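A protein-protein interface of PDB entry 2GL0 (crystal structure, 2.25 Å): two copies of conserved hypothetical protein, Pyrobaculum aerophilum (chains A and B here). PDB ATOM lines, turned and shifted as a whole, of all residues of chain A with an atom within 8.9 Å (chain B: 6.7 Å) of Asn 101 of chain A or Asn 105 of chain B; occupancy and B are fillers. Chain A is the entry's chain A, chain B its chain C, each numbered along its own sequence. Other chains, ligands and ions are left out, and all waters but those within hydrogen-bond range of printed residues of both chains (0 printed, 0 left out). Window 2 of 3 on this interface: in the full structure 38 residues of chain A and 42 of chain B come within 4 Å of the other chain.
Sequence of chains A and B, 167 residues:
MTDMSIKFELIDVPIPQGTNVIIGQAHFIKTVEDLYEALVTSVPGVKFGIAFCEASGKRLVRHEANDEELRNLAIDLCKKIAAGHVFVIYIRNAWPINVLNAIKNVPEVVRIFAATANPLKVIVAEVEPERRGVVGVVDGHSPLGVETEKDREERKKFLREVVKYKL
Of the 10 printed residues of chain B, 6 touch a printed residue of chain A.
Printed residues of chain B that touch a printed residue of chain A: Lys 104, Asn 105, Val 106, Pro 107, Glu 108 and Val 109.
Of the 18 printed residues of chain A, 4 touch a printed residue of chain B.
Printed residues of chain A that touch a printed residue of chain B: Ile 97, Leu 100, Asn 101 and Lys 104.
Hydrophobic or aromatic side chains of chain A that line the printed part of chain B: Ile 97 and Leu 100.
Among the printed residues, 8 pairs touch across the chains.
The side-chain amide nitrogen (ND2) of Asn 101 of chain A sits at hydrogen-bond distance from the backbone carbonyl oxygen (O) of Asn 105 of chain B (2.9 Å).
The backbone carbonyl oxygen of Val 109 of chain B sits at hydrogen-bond distance from the side-chain amino group of Lys 104 of chain A (3.0 Å).
NZ of Lys 104 of chain A sits at hydrogen-bond distance from O of Lys 104 of chain B.
The backbone carbonyl oxygen (O) of Val 106 of chain B lies within hydrogen-bond range of the side-chain amino group (NZ) of Lys 104 of chain A, at 3.2 Å.
The backbone carbonyl oxygen (O) of Asn 101 of chain B lies within hydrogen-bond range of the side-chain amide nitrogen (ND2) of Asn 105 of chain B (3.3 Å).
O of Asn 101 of chain A lies close to OD1 of Asn 105 of chain A, at 2.9 Å.
The side-chain amide oxygen (OD1) of Asn 101 of chain A lies within hydrogen-bond range of the side-chain amino group (NZ) of Lys 104 of chain A (2.7 Å).
The side-chain amide oxygen (OD1) of Asn 101 of chain B lies within hydrogen-bond range of the side-chain amino group (NZ) of Lys 104 of chain B (2.9 Å).
Ile 97 of chain A touches Pro 107 of chain B (O to CB, 3.7 Å).
Glu 108 of chain B touches Ile 97 of chain A (OE2 to CG2, 3.6 Å).
CD1 of Leu 100 of chain A touches O of Pro 107 of chain B (3.5 Å).
Asn 101 of chain A touches Pro 107 of chain B.
Leu 100 of chain A touches Pro 107 of chain B, but with the chains exchanged Pro 107 of chain A does not touch Leu 100 of chain B (17.9 Å).
Asn 101 of chain A touches Asn 105 of chain B, but with the chains exchanged Asn 105 of chain A does not touch Asn 101 of chain B (9.6 Å).
Asn 101 of chain A touches Pro 107 of chain B, but with the chains exchanged Pro 107 of chain A does not touch Asn 101 of chain B (15.5 Å).
Lys 104 of chain A touches its own counterpart, Lys 104 of chain B.
Positions printed for both chains: 100, 101, 102, 103, 104, 105, 106, 107 and 109.
Of the 8 pairs that touch across the chains among the printed residues, 1 has its exchanged pair printed and touching as well.
Of the printed residues of chain B, Ile 97 of chain A touches Pro 107 (3.7 Å) and Glu 108 (3.6 Å).
Printed residues of chain B within 4 Å of Leu 100 of chain A: Pro 107 (3.5 Å).
Printed residues of chain B within 4 Å of Asn 101 of chain A: Asn 105 and Pro 107.
Of the printed residues of chain B, Lys 104 of chain A touches Lys 104, Val 106 and Val 109.
Ile 112 of chain A touches none of the printed residues of chain B.
Printed residues of chain A within 4 Å of Val 109 of chain B: Lys 104.
The nearest printed residue of chain A that does not touch Val 109 of chain B is Leu 100 of chain A (5.1 Å).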
ATOM      1  N   ILE A  22      19.686 -30.121  10.022  1.00  0.00           N
ATOM      2  CA  ILE A  22      20.255 -29.462   8.866  1.00  0.00           C
ATOM      3  C   ILE A  22      19.062 -29.061   7.988  1.00  0.00           C
ATOM      4  O   ILE A  22      18.205 -29.894   7.688  1.00  0.00           O
ATOM      5  CB  ILE A  22      21.241 -30.373   8.098  1.00  0.00           C
ATOM      6  CG1 ILE A  22      22.383 -30.876   9.039  1.00  0.00           C
ATOM      7  CG2 ILE A  22      21.723 -29.636   6.806  1.00  0.00           C
ATOM      8  CD1 ILE A  22      23.294 -31.825   8.455  1.00  0.00           C
ATOM      9  N   ALA A  38      23.855 -39.608   0.721  1.00  0.00           N
ATOM     10  CA  ALA A  38      24.943 -38.711   1.231  1.00  0.00           C
ATOM     11  C   ALA A  38      25.106 -38.905   2.744  1.00  0.00           C
ATOM     12  O   ALA A  38      26.255 -38.970   3.297  1.00  0.00           O
ATOM     13  CB  ALA A  38      24.685 -37.242   0.828  1.00  0.00           C
ATOM     14  N   SER A  42      28.308 -41.424   4.705  1.00  0.00           N
ATOM     15  CA  SER A  42      29.232 -40.545   5.393  1.00  0.00           C
ATOM     16  C   SER A  42      29.756 -41.141   6.730  1.00  0.00           C
ATOM     17  O   SER A  42      30.906 -40.927   7.094  1.00  0.00           O
ATOM     18  CB  SER A  42      28.544 -39.200   5.722  1.00  0.00           C
ATOM     19  OG  SER A  42      28.176 -38.596   4.502  1.00  0.00           O
ATOM     20  N   TRP A  95      27.721 -35.766  13.645  1.00  0.00           N
ATOM     21  CA  TRP A  95      27.734 -34.316  13.792  1.00  0.00           C
ATOM     22  C   TRP A  95      27.592 -33.816  12.373  1.00  0.00           C
ATOM     23  O   TRP A  95      28.040 -34.551  11.443  1.00  0.00           O
ATOM     24  CB  TRP A  95      29.105 -33.890  14.285  1.00  0.00           C
ATOM     25  CG  TRP A  95      29.424 -34.257  15.735  1.00  0.00           C
ATOM     26  CD1 TRP A  95      30.408 -35.077  16.157  1.00  0.00           C
ATOM     27  CD2 TRP A  95      28.755 -33.789  16.922  1.00  0.00           C
ATOM     28  NE1 TRP A  95      30.410 -35.154  17.495  1.00  0.00           N
ATOM     29  CE2 TRP A  95      29.418 -34.365  18.009  1.00  0.00           C
ATOM     30  CE3 TRP A  95      27.690 -32.930  17.160  1.00  0.00           C
ATOM     31  CZ2 TRP A  95      29.019 -34.156  19.338  1.00  0.00           C
ATOM     32  CZ3 TRP A  95      27.302 -32.677  18.467  1.00  0.00           C
ATOM     33  CH2 TRP A  95      27.948 -33.308  19.547  1.00  0.00           C
ATOM     34  N   PRO A  96      26.944 -32.615  12.185  1.00  0.00           N
ATOM     35  CA  PRO A  96      26.877 -31.925  10.846  1.00  0.00           C
ATOM     36  C   PRO A  96      28.175 -31.827  10.114  1.00  0.00           C
ATOM     37  O   PRO A  96      28.197 -32.255   8.998  1.00  0.00           O
ATOM     38  CB  PRO A  96      26.233 -30.572  11.155  1.00  0.00           C
ATOM     39  CG  PRO A  96      25.328 -30.953  12.413  1.00  0.00           C
ATOM     40  CD  PRO A  96      26.172 -31.889  13.217  1.00  0.00           C
ATOM     41  N   ILE A  97      29.282 -31.474  10.768  1.00  0.00           N
ATOM     42  CA  ILE A  97      30.595 -31.432  10.098  1.00  0.00           C
ATOM     43  C   ILE A  97      30.997 -32.762   9.486  1.00  0.00           C
ATOM     44  O   ILE A  97      31.795 -32.740   8.580  1.00  0.00           O
ATOM     45  CB  ILE A  97      31.800 -30.908  10.998  1.00  0.00           C
ATOM     46  CG1 ILE A  97      32.174 -31.917  12.151  1.00  0.00           C
ATOM     47  CG2 ILE A  97      31.545 -29.401  11.472  1.00  0.00           C
ATOM     48  CD1 ILE A  97      33.498 -31.571  13.102  1.00  0.00           C
ATOM     49  N   ASN A  98      30.488 -33.902  10.017  1.00  0.00           N
ATOM     50  CA  ASN A  98      30.723 -35.237   9.370  1.00  0.00           C
ATOM     51  C   ASN A  98      30.099 -35.440   8.045  1.00  0.00           C
ATOM     52  O   ASN A  98      30.579 -36.321   7.353  1.00  0.00           O
ATOM     53  CB  ASN A  98      30.253 -36.477  10.161  1.00  0.00           C
ATOM     54  CG  ASN A  98      30.687 -36.489  11.611  1.00  0.00           C
ATOM     55  OD1 ASN A  98      29.958 -37.048  12.450  1.00  0.00           O
ATOM     56  ND2 ASN A  98      31.880 -35.920  11.925  1.00  0.00           N
ATOM     57  N   VAL A  99      29.066 -34.670   7.673  1.00  0.00           N
ATOM     58  CA  VAL A  99      28.162 -35.014   6.489  1.00  0.00           C
ATOM     59  C   VAL A  99      27.922 -33.846   5.595  1.00  0.00           C
ATOM     60  O   VAL A  99      27.348 -34.010   4.500  1.00  0.00           O
ATOM     61  CB  VAL A  99      26.743 -35.562   6.953  1.00  0.00           C
ATOM     62  CG1 VAL A  99      26.874 -36.933   7.646  1.00  0.00           C
ATOM     63  CG2 VAL A  99      26.050 -34.592   7.914  1.00  0.00           C
ATOM     64  N   LEU A 100      28.352 -32.645   6.038  1.00  0.00           N
ATOM     65  CA  LEU A 100      27.968 -31.415   5.380  1.00  0.00           C
ATOM     66  C   LEU A 100      28.541 -31.204   3.997  1.00  0.00           C
ATOM     67  O   LEU A 100      27.837 -30.747   3.078  1.00  0.00           O
ATOM     68  CB  LEU A 100      28.205 -30.176   6.257  1.00  0.00           C
ATOM     69  CG  LEU A 100      26.923 -29.678   6.978  1.00  0.00           C
ATOM     70  CD1 LEU A 100      27.357 -28.783   8.083  1.00  0.00           C
ATOM     71  CD2 LEU A 100      26.031 -28.934   6.011  1.00  0.00           C
ATOM     72  N   ASN A 101      29.838 -31.441   3.844  1.00  0.00           N
ATOM     73  CA  ASN A 101      30.448 -31.153   2.527  1.00  0.00           C
ATOM     74  C   ASN A 101      29.808 -32.038   1.461  1.00  0.00           C
ATOM     75  O   ASN A 101      29.613 -31.586   0.329  1.00  0.00           O
ATOM     76  CB  ASN A 101      31.976 -31.286   2.561  1.00  0.00           C
ATOM     77  CG  ASN A 101      32.649 -30.011   3.058  1.00  0.00           C
ATOM     78  OD1 ASN A 101      31.980 -29.033   3.350  1.00  0.00           O
ATOM     79  ND2 ASN A 101      33.986 -30.020   3.143  1.00  0.00           N
ATOM     80  N   ALA A 102      29.460 -33.280   1.851  1.00  0.00           N
ATOM     81  CA  ALA A 102      28.755 -34.198   1.033  1.00  0.00           C
ATOM     82  C   ALA A 102      27.361 -33.624   0.627  1.00  0.00           C
ATOM     83  O   ALA A 102      26.955 -33.705  -0.548  1.00  0.00           O
ATOM     84  CB  ALA A 102      28.627 -35.598   1.759  1.00  0.00           C
ATOM     85  N   ILE A 103      26.641 -33.056   1.589  1.00  0.00           N
ATOM     86  CA  ILE A 103      25.329 -32.484   1.302  1.00  0.00           C
ATOM     87  C   ILE A 103      25.476 -31.362   0.286  1.00  0.00           C
ATOM     88  O   ILE A 103      24.725 -31.305  -0.633  1.00  0.00           O
ATOM     89  CB  ILE A 103      24.558 -31.997   2.598  1.00  0.00           C
ATOM     90  CG1 ILE A 103      24.294 -33.155   3.520  1.00  0.00           C
ATOM     91  CG2 ILE A 103      23.211 -31.239   2.197  1.00  0.00           C
ATOM     92  CD1 ILE A 103      23.619 -32.813   4.694  1.00  0.00           C
ATOM     93  N   LYS A 104      26.507 -30.525   0.456  1.00  0.00           N
ATOM     94  CA  LYS A 104      26.770 -29.334  -0.354  1.00  0.00           C
ATOM     95  C   LYS A 104      26.948 -29.766  -1.771  1.00  0.00           C
ATOM     96  O   LYS A 104      26.633 -29.007  -2.696  1.00  0.00           O
ATOM     97  CB  LYS A 104      28.064 -28.597   0.098  1.00  0.00           C
ATOM     98  CG  LYS A 104      27.948 -27.880   1.490  1.00  0.00           C
ATOM     99  CD  LYS A 104      29.288 -27.347   1.873  1.00  0.00           C
ATOM    100  CE  LYS A 104      29.411 -27.116   3.308  1.00  0.00           C
ATOM    101  NZ  LYS A 104      30.790 -26.571   3.641  1.00  0.00           N
ATOM    102  N   ASN A 105      27.468 -30.983  -1.944  1.00  0.00           N
ATOM    103  CA  ASN A 105      27.740 -31.541  -3.299  1.00  0.00           C
ATOM    104  C   ASN A 105      26.666 -32.334  -4.046  1.00  0.00           C
ATOM    105  O   ASN A 105      26.935 -32.857  -5.106  1.00  0.00           O
ATOM    106  CB  ASN A 105      28.969 -32.388  -3.282  1.00  0.00           C
ATOM    107  CG  ASN A 105      30.130 -31.575  -3.377  1.00  0.00           C
ATOM    108  OD1 ASN A 105      30.776 -31.249  -2.316  1.00  0.00           O
ATOM    109  ND2 ASN A 105      30.420 -31.109  -4.633  1.00  0.00           N
ATOM    110  N   VAL A 106      25.476 -32.391  -3.490  1.00  0.00           N
ATOM    111  CA  VAL A 106      24.367 -33.137  -4.121  1.00  0.00           C
ATOM    112  C   VAL A 106      23.935 -32.155  -5.193  1.00  0.00           C
ATOM    113  O   VAL A 106      23.662 -30.986  -4.830  1.00  0.00           O
ATOM    114  CB  VAL A 106      23.239 -33.315  -3.075  1.00  0.00           C
ATOM    115  CG1 VAL A 106      22.140 -34.148  -3.584  1.00  0.00           C
ATOM    116  CG2 VAL A 106      23.809 -33.984  -1.884  1.00  0.00           C
ATOM    117  N   PRO A 107      24.023 -32.527  -6.487  1.00  0.00           N
ATOM    118  CA  PRO A 107      23.642 -31.651  -7.585  1.00  0.00           C
ATOM    119  C   PRO A 107      22.325 -30.803  -7.428  1.00  0.00           C
ATOM    120  O   PRO A 107      22.300 -29.658  -7.800  1.00  0.00           O
ATOM    121  CB  PRO A 107      23.589 -32.641  -8.751  1.00  0.00           C
ATOM    122  CG  PRO A 107      24.807 -33.508  -8.513  1.00  0.00           C
ATOM    123  CD  PRO A 107      24.614 -33.753  -6.985  1.00  0.00           C
ATOM    124  N   VAL A 109      21.026 -29.756  -4.453  1.00  0.00           N
ATOM    125  CA  VAL A 109      21.133 -28.802  -3.315  1.00  0.00           C
ATOM    126  C   VAL A 109      21.646 -27.389  -3.776  1.00  0.00           C
ATOM    127  O   VAL A 109      22.743 -27.231  -4.338  1.00  0.00           O
ATOM    128  CB  VAL A 109      21.947 -29.452  -2.090  1.00  0.00           C
ATOM    129  CG1 VAL A 109      22.310 -28.452  -1.038  1.00  0.00           C
ATOM    130  CG2 VAL A 109      21.117 -30.592  -1.515  1.00  0.00           C
ATOM    131  N   ILE A 112      22.102 -24.139   1.957  1.00  0.00           N
ATOM    132  CA  ILE A 112      21.883 -24.651   3.306  1.00  0.00           C
ATOM    133  C   ILE A 112      21.599 -23.395   4.220  1.00  0.00           C
ATOM    134  O   ILE A 112      22.321 -22.373   4.205  1.00  0.00           O
ATOM    135  CB  ILE A 112      23.011 -25.582   3.817  1.00  0.00           C
ATOM    136  CG1 ILE A 112      23.315 -26.765   2.816  1.00  0.00           C
ATOM    137  CG2 ILE A 112      22.555 -26.268   5.158  1.00  0.00           C
ATOM    138  CD1 ILE A 112      24.642 -27.347   2.989  1.00  0.00           C
ATOM    139  N   LEU B 100      37.751 -17.742  -1.476  1.00  0.00           N
ATOM    140  CA  LEU B 100      36.336 -18.086  -1.330  1.00  0.00           C
ATOM    141  C   LEU B 100      36.101 -19.597  -1.359  1.00  0.00           C
ATOM    142  O   LEU B 100      35.523 -20.116  -0.452  1.00  0.00           O
ATOM    143  CB  LEU B 100      35.543 -17.365  -2.353  1.00  0.00           C
ATOM    144  CG  LEU B 100      34.258 -16.722  -1.829  1.00  0.00           C
ATOM    145  CD1 LEU B 100      34.265 -16.368  -0.364  1.00  0.00           C
ATOM    146  CD2 LEU B 100      33.933 -15.483  -2.736  1.00  0.00           C
ATOM    147  N   ASN B 101      36.632 -20.310  -2.359  1.00  0.00           N
ATOM    148  CA  ASN B 101      36.428 -21.745  -2.456  1.00  0.00           C
ATOM    149  C   ASN B 101      36.906 -22.539  -1.251  1.00  0.00           C
ATOM    150  O   ASN B 101      36.207 -23.416  -0.834  1.00  0.00           O
ATOM    151  CB  ASN B 101      36.955 -22.294  -3.790  1.00  0.00           C
ATOM    152  CG  ASN B 101      36.049 -21.934  -4.978  1.00  0.00           C
ATOM    153  OD1 ASN B 101      35.002 -21.252  -4.849  1.00  0.00           O
ATOM    154  ND2 ASN B 101      36.430 -22.413  -6.135  1.00  0.00           N
ATOM    155  N   ALA B 102      38.085 -22.244  -0.705  1.00  0.00           N
ATOM    156  CA  ALA B 102      38.533 -22.834   0.549  1.00  0.00           C
ATOM    157  C   ALA B 102      37.494 -22.658   1.713  1.00  0.00           C
ATOM    158  O   ALA B 102      37.268 -23.593   2.447  1.00  0.00           O
ATOM    159  CB  ALA B 102      39.872 -22.297   0.962  1.00  0.00           C
ATOM    160  N   ILE B 103      36.951 -21.450   1.850  1.00  0.00           N
ATOM    161  CA  ILE B 103      35.960 -21.053   2.843  1.00  0.00           C
ATOM    162  C   ILE B 103      34.674 -21.813   2.662  1.00  0.00           C
ATOM    163  O   ILE B 103      34.129 -22.206   3.662  1.00  0.00           O
ATOM    164  CB  ILE B 103      35.700 -19.591   2.782  1.00  0.00           C
ATOM    165  CG1 ILE B 103      36.945 -18.787   3.274  1.00  0.00           C
ATOM    166  CG2 ILE B 103      34.482 -19.188   3.705  1.00  0.00           C
ATOM    167  CD1 ILE B 103      36.939 -17.266   2.750  1.00  0.00           C
ATOM    168  N   LYS B 104      34.219 -22.053   1.402  1.00  0.00           N
ATOM    169  CA  LYS B 104      33.058 -22.910   1.033  1.00  0.00           C
ATOM    170  C   LYS B 104      33.123 -24.328   1.598  1.00  0.00           C
ATOM    171  O   LYS B 104      32.124 -24.901   1.993  1.00  0.00           O
ATOM    172  CB  LYS B 104      32.894 -22.994  -0.499  1.00  0.00           C
ATOM    173  CG  LYS B 104      32.367 -21.684  -1.136  1.00  0.00           C
ATOM    174  CD  LYS B 104      32.409 -21.767  -2.734  1.00  0.00           C
ATOM    175  CE  LYS B 104      32.298 -20.417  -3.454  1.00  0.00           C
ATOM    176  NZ  LYS B 104      32.212 -20.437  -5.006  1.00  0.00           N
ATOM    177  N   ASN B 105      34.320 -24.884   1.617  1.00  0.00           N
ATOM    178  CA  ASN B 105      34.546 -26.249   1.892  1.00  0.00           C
ATOM    179  C   ASN B 105      35.029 -26.492   3.320  1.00  0.00           C
ATOM    180  O   ASN B 105      35.487 -27.566   3.668  1.00  0.00           O
ATOM    181  CB  ASN B 105      35.631 -26.705   0.900  1.00  0.00           C
ATOM    182  CG  ASN B 105      35.023 -27.243  -0.412  1.00  0.00           C
ATOM    183  OD1 ASN B 105      34.434 -28.310  -0.429  1.00  0.00           O
ATOM    184  ND2 ASN B 105      35.139 -26.481  -1.474  1.00  0.00           N
ATOM    185  N   VAL B 106      34.920 -25.479   4.155  1.00  0.00           N
ATOM    186  CA  VAL B 106      35.233 -25.660   5.561  1.00  0.00           C
ATOM    187  C   VAL B 106      33.993 -26.341   6.042  1.00  0.00           C
ATOM    188  O   VAL B 106      32.949 -25.785   5.865  1.00  0.00           O
ATOM    189  CB  VAL B 106      35.551 -24.259   6.246  1.00  0.00           C
ATOM    190  CG1 VAL B 106      35.300 -24.304   7.722  1.00  0.00           C
ATOM    191  CG2 VAL B 106      37.039 -23.924   6.050  1.00  0.00           C
ATOM    192  N   PRO B 107      34.093 -27.583   6.637  1.00  0.00           N
ATOM    193  CA  PRO B 107      32.864 -28.294   7.072  1.00  0.00           C
ATOM    194  C   PRO B 107      31.880 -27.505   8.006  1.00  0.00           C
ATOM    195  O   PRO B 107      30.688 -27.764   7.967  1.00  0.00           O
ATOM    196  CB  PRO B 107      33.412 -29.509   7.707  1.00  0.00           C
ATOM    197  CG  PRO B 107      34.743 -29.762   6.837  1.00  0.00           C
ATOM    198  CD  PRO B 107      35.304 -28.426   6.874  1.00  0.00           C
ATOM    199  N   GLU B 108      32.354 -26.532   8.764  1.00  0.00           N
ATOM    200  CA  GLU B 108      31.481 -25.858   9.692  1.00  0.00           C
ATOM    201  C   GLU B 108      30.615 -24.806   8.890  1.00  0.00           C
ATOM    202  O   GLU B 108      29.483 -24.503   9.301  1.00  0.00           O
ATOM    203  CB  GLU B 108      32.287 -25.179  10.797  1.00  0.00           C
ATOM    204  CG  GLU B 108      32.907 -26.081  11.962  1.00  0.00           C
ATOM    205  CD  GLU B 108      34.244 -26.677  11.620  1.00  0.00           C
ATOM    206  OE1 GLU B 108      34.965 -26.112  10.789  1.00  0.00           O
ATOM    207  OE2 GLU B 108      34.606 -27.731  12.144  1.00  0.00           O
ATOM    208  N   VAL B 109      31.149 -24.317   7.761  1.00  0.00           N
ATOM    209  CA  VAL B 109      30.485 -23.240   6.949  1.00  0.00           C
ATOM    210  C   VAL B 109      29.206 -23.767   6.259  1.00  0.00           C
ATOM    211  O   VAL B 109      29.288 -24.779   5.542  1.00  0.00           O
ATOM    212  CB  VAL B 109      31.445 -22.617   5.877  1.00  0.00           C
ATOM    213  CG1 VAL B 109      30.586 -21.748   4.902  1.00  0.00           C
ATOM    214  CG2 VAL B 109      32.632 -21.826   6.585  1.00  0.00           C
